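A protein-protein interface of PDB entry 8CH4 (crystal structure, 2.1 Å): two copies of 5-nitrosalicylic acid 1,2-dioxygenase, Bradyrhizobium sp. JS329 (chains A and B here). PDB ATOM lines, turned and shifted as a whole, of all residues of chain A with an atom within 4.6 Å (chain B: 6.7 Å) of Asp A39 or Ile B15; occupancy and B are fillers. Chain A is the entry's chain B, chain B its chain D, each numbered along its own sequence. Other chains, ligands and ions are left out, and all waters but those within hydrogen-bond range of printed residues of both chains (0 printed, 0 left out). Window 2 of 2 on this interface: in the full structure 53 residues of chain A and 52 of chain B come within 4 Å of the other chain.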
ATOM      1  N   TRP A  35      18.283  -3.407  -4.530  1.00  0.00           N
ATOM      2  CA  TRP A  35      18.969  -4.593  -4.058  1.00  0.00           C
ATOM      3  C   TRP A  35      18.731  -5.687  -5.088  1.00  0.00           C
ATOM      4  O   TRP A  35      17.617  -5.802  -5.599  1.00  0.00           O
ATOM      5  CB  TRP A  35      18.468  -5.010  -2.662  1.00  0.00           C
ATOM      6  CG  TRP A  35      18.599  -3.901  -1.663  1.00  0.00           C
ATOM      7  CD1 TRP A  35      19.636  -3.670  -0.798  1.00  0.00           C
ATOM      8  CD2 TRP A  35      17.684  -2.804  -1.486  1.00  0.00           C
ATOM      9  NE1 TRP A  35      19.414  -2.523  -0.079  1.00  0.00           N
ATOM     10  CE2 TRP A  35      18.230  -1.965  -0.490  1.00  0.00           C
ATOM     11  CE3 TRP A  35      16.469  -2.448  -2.082  1.00  0.00           C
ATOM     12  CZ2 TRP A  35      17.589  -0.799  -0.074  1.00  0.00           C
ATOM     13  CZ3 TRP A  35      15.833  -1.301  -1.661  1.00  0.00           C
ATOM     14  CH2 TRP A  35      16.385  -0.492  -0.665  1.00  0.00           C
ATOM     15  N   GLU A  36      19.783  -6.474  -5.370  1.00  0.00           N
ATOM     16  CA  GLU A  36      19.697  -7.591  -6.301  1.00  0.00           C
ATOM     17  C   GLU A  36      19.616  -8.884  -5.507  1.00  0.00           C
ATOM     18  O   GLU A  36      20.378  -9.074  -4.570  1.00  0.00           O
ATOM     19  CB  GLU A  36      20.916  -7.633  -7.222  1.00  0.00           C
ATOM     20  CG  GLU A  36      21.257  -6.283  -7.822  1.00  0.00           C
ATOM     21  CD  GLU A  36      21.714  -6.268  -9.275  1.00  0.00           C
ATOM     22  OE1 GLU A  36      21.674  -5.126  -9.886  1.00  0.00           O
ATOM     23  OE2 GLU A  36      22.089  -7.379  -9.809  1.00  0.00           O
ATOM     24  N   TRP A  37      18.722  -9.784  -5.925  1.00  0.00           N
ATOM     25  CA  TRP A  37      18.492 -11.031  -5.218  1.00  0.00           C
ATOM     26  C   TRP A  37      19.807 -11.763  -4.949  1.00  0.00           C
ATOM     27  O   TRP A  37      19.963 -12.439  -3.929  1.00  0.00           O
ATOM     28  CB  TRP A  37      17.501 -11.904  -5.988  1.00  0.00           C
ATOM     29  CG  TRP A  37      16.997 -13.059  -5.177  1.00  0.00           C
ATOM     30  CD1 TRP A  37      17.122 -14.385  -5.474  1.00  0.00           C
ATOM     31  CD2 TRP A  37      16.296 -12.996  -3.916  1.00  0.00           C
ATOM     32  NE1 TRP A  37      16.525 -15.147  -4.499  1.00  0.00           N
ATOM     33  CE2 TRP A  37      16.012 -14.322  -3.530  1.00  0.00           C
ATOM     34  CE3 TRP A  37      15.853 -11.954  -3.088  1.00  0.00           C
ATOM     35  CZ2 TRP A  37      15.328 -14.627  -2.350  1.00  0.00           C
ATOM     36  CZ3 TRP A  37      15.180 -12.258  -1.921  1.00  0.00           C
ATOM     37  CH2 TRP A  37      14.927 -13.579  -1.553  1.00  0.00           C
ATOM     38  N   ALA A  38      20.751 -11.623  -5.882  1.00  0.00           N
ATOM     39  CA  ALA A  38      22.006 -12.348  -5.830  1.00  0.00           C
ATOM     40  C   ALA A  38      22.842 -11.857  -4.647  1.00  0.00           C
ATOM     41  O   ALA A  38      23.599 -12.627  -4.059  1.00  0.00           O
ATOM     42  CB  ALA A  38      22.739 -12.229  -7.147  1.00  0.00           C
ATOM     43  N   ASP A  39      22.687 -10.585  -4.279  1.00  0.00           N
ATOM     44  CA  ASP A  39      23.455 -10.059  -3.164  1.00  0.00           C
ATOM     45  C   ASP A  39      22.871 -10.609  -1.871  1.00  0.00           C
ATOM     46  O   ASP A  39      23.599 -10.836  -0.908  1.00  0.00           O
ATOM     47  CB  ASP A  39      23.543  -8.534  -3.206  1.00  0.00           C
ATOM     48  CG  ASP A  39      24.277  -8.025  -4.438  1.00  0.00           C
ATOM     49  OD1 ASP A  39      25.287  -8.643  -4.806  1.00  0.00           O
ATOM     50  OD2 ASP A  39      23.831  -7.015  -5.021  1.00  0.00           O
ATOM     51  N   VAL A  40      21.555 -10.849  -1.896  1.00  0.00           N
ATOM     52  CA  VAL A  40      20.808 -11.281  -0.726  1.00  0.00           C
ATOM     53  C   VAL A  40      21.228 -12.716  -0.438  1.00  0.00           C
ATOM     54  O   VAL A  40      21.662 -13.041   0.665  1.00  0.00           O
ATOM     55  CB  VAL A  40      19.274 -11.142  -0.917  1.00  0.00           C
ATOM     56  CG1 VAL A  40      18.477 -11.822   0.187  1.00  0.00           C
ATOM     57  CG2 VAL A  40      18.829  -9.688  -1.041  1.00  0.00           C
ATOM     58  N   VAL A  41      21.106 -13.547  -1.475  1.00  0.00           N
ATOM     59  CA  VAL A  41      21.409 -14.971  -1.424  1.00  0.00           C
ATOM     60  C   VAL A  41      22.881 -15.217  -1.090  1.00  0.00           C
ATOM     61  O   VAL A  41      23.180 -16.098  -0.295  1.00  0.00           O
ATOM     62  CB  VAL A  41      20.973 -15.643  -2.734  1.00  0.00           C
ATOM     63  CG1 VAL A  41      21.649 -16.993  -2.939  1.00  0.00           C
ATOM     64  CG2 VAL A  41      19.451 -15.754  -2.783  1.00  0.00           C
ATOM     65  N   SER A  42      23.786 -14.436  -1.681  1.00  0.00           N
ATOM     66  CA  SER A  42      25.193 -14.501  -1.324  1.00  0.00           C
ATOM     67  C   SER A  42      25.362 -14.224   0.171  1.00  0.00           C
ATOM     68  O   SER A  42      25.917 -15.049   0.888  1.00  0.00           O
ATOM     69  CB  SER A  42      26.021 -13.582  -2.173  1.00  0.00           C
ATOM     70  OG  SER A  42      27.123 -13.064  -1.442  1.00  0.00           O
ATOM     71  N   GLY A  43      24.851 -13.074   0.636  1.00  0.00           N
ATOM     72  CA  GLY A  43      24.781 -12.738   2.055  1.00  0.00           C
ATOM     73  C   GLY A  43      24.273 -13.879   2.949  1.00  0.00           C
ATOM     74  O   GLY A  43      24.841 -14.146   4.018  1.00  0.00           O
ATOM     75  N   VAL A  60      19.071 -11.750   6.932  1.00  0.00           N
ATOM     76  CA  VAL A  60      19.741 -10.485   6.676  1.00  0.00           C
ATOM     77  C   VAL A  60      18.684  -9.383   6.632  1.00  0.00           C
ATOM     78  O   VAL A  60      17.512  -9.624   6.313  1.00  0.00           O
ATOM     79  CB  VAL A  60      20.514 -10.512   5.341  1.00  0.00           C
ATOM     80  CG1 VAL A  60      21.848 -11.216   5.467  1.00  0.00           C
ATOM     81  CG2 VAL A  60      19.690 -11.094   4.190  1.00  0.00           C
ATOM     82  N   ALA A  61      19.120  -8.158   6.935  1.00  0.00           N
ATOM     83  CA  ALA A  61      18.241  -7.009   6.797  1.00  0.00           C
ATOM     84  C   ALA A  61      18.634  -6.225   5.545  1.00  0.00           C
ATOM     85  O   ALA A  61      19.802  -5.874   5.358  1.00  0.00           O
ATOM     86  CB  ALA A  61      18.299  -6.160   8.037  1.00  0.00           C
ATOM     87  N   SER B  13      22.484   1.188  -0.697  1.00  0.00           N
ATOM     88  CA  SER B  13      21.611   0.028  -0.586  1.00  0.00           C
ATOM     89  C   SER B  13      22.397  -1.172  -0.051  1.00  0.00           C
ATOM     90  O   SER B  13      23.108  -1.835  -0.787  1.00  0.00           O
ATOM     91  CB  SER B  13      20.965  -0.277  -1.914  1.00  0.00           C
ATOM     92  OG  SER B  13      19.982   0.698  -2.226  1.00  0.00           O
ATOM     93  N   LYS B  14      22.262  -1.474   1.241  1.00  0.00           N
ATOM     94  CA  LYS B  14      23.103  -2.504   1.819  1.00  0.00           C
ATOM     95  C   LYS B  14      22.283  -3.680   2.323  1.00  0.00           C
ATOM     96  O   LYS B  14      21.060  -3.611   2.441  1.00  0.00           O
ATOM     97  CB  LYS B  14      23.991  -1.954   2.928  1.00  0.00           C
ATOM     98  CG  LYS B  14      24.856  -0.793   2.477  1.00  0.00           C
ATOM     99  CD  LYS B  14      26.120  -0.738   3.292  1.00  0.00           C
ATOM    100  CE  LYS B  14      27.103   0.274   2.761  1.00  0.00           C
ATOM    101  NZ  LYS B  14      27.482   1.196   3.851  1.00  0.00           N
ATOM    102  N   ILE B  15      23.010  -4.771   2.573  1.00  0.00           N
ATOM    103  CA  ILE B  15      22.503  -5.953   3.238  1.00  0.00           C
ATOM    104  C   ILE B  15      23.328  -6.154   4.509  1.00  0.00           C
ATOM    105  O   ILE B  15      24.550  -6.173   4.458  1.00  0.00           O
ATOM    106  CB  ILE B  15      22.577  -7.146   2.271  1.00  0.00           C
ATOM    107  CG1 ILE B  15      21.799  -6.823   0.988  1.00  0.00           C
ATOM    108  CG2 ILE B  15      22.072  -8.407   2.958  1.00  0.00           C
ATOM    109  CD1 ILE B  15      22.043  -7.759  -0.164  1.00  0.00           C
ATOM    110  N   ILE B  16      22.653  -6.216   5.666  1.00  0.00           N
ATOM    111  CA  ILE B  16      23.371  -6.366   6.918  1.00  0.00           C
ATOM    112  C   ILE B  16      22.915  -7.646   7.619  1.00  0.00           C
ATOM    113  O   ILE B  16      21.807  -8.150   7.393  1.00  0.00           O
ATOM    114  CB  ILE B  16      23.296  -5.089   7.782  1.00  0.00           C
ATOM    115  CG1 ILE B  16      21.883  -4.833   8.314  1.00  0.00           C
ATOM    116  CG2 ILE B  16      23.845  -3.878   7.024  1.00  0.00           C
ATOM    117  CD1 ILE B  16      21.782  -3.635   9.239  1.00  0.00           C
ATOM    118  N   HIS B  17      23.856  -8.172   8.411  1.00  0.00           N
ATOM    119  CA  HIS B  17      23.760  -9.311   9.310  1.00  0.00           C
ATOM    120  C   HIS B  17      22.758  -9.017  10.439  1.00  0.00           C
ATOM    121  O   HIS B  17      22.845  -7.972  11.090  1.00  0.00           O
ATOM    122  CB  HIS B  17      25.184  -9.505   9.861  1.00  0.00           C
ATOM    123  CG  HIS B  17      25.419 -10.696  10.724  1.00  0.00           C
ATOM    124  ND1 HIS B  17      24.647 -10.982  11.837  1.00  0.00           N
ATOM    125  CD2 HIS B  17      26.379 -11.645  10.676  1.00  0.00           C
ATOM    126  CE1 HIS B  17      25.092 -12.078  12.416  1.00  0.00           C
ATOM    127  NE2 HIS B  17      26.156 -12.504  11.722  1.00  0.00           N
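O of Lys B14 is in hydrogen-bond range of NE1 of Trp A35, at 3.2 Å.
N of Ala A61 lies within hydrogen-bond range of O of Ile B16 (2.7 Å).
Among the printed residues, merely in contact across the chains: Trp A35 with Ser B13, Asp A39 with Ile B15, Val A40 with Ile B15, Val A60 with Ile B15, Val A60 with Ile B16, Ala A61 with Lys B14 and Ala A61 with Ile B15.
Trp A37 touches none of the printed residues of chain B.
Ala A38 touches none of the printed residues of chain B.
Of chain B, only Ile B15 (3.4 Å) comes within 4 Å of Asp A39.
Of the printed residues of chain B, Val A40 touches Ile B15.
Of the printed residues of chain B, Val A60 touches Ile B15 (3.5 Å) and Ile B16 (3.2 Å).
Printed residues of chain A within 4 Å of Ile B15: Asp A39 (3.4 Å), Val A40 (3.6 Å), Val A60 (3.5 Å) and Ala A61 (3.4 Å).
The nearest residue of chain A that does not touch Ile B15 is Trp A35 (4.2 Å).
The nearest printed residue of chain B that does not touch Trp A35 is Ile B15 (4.2 Å).
Hydrophobic or aromatic side chains of chain B that line the printed part of chain A: Ile B15 and Ile B16.
Along chain A the printed residues that touch a printed residue of chain B span positions 35 to 61.
Among the printed residues, no Asp or Glu carboxylate lies within 4 Å of a Lys or Arg side-chain nitrogen of the other chain.
No position is printed for both chains.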
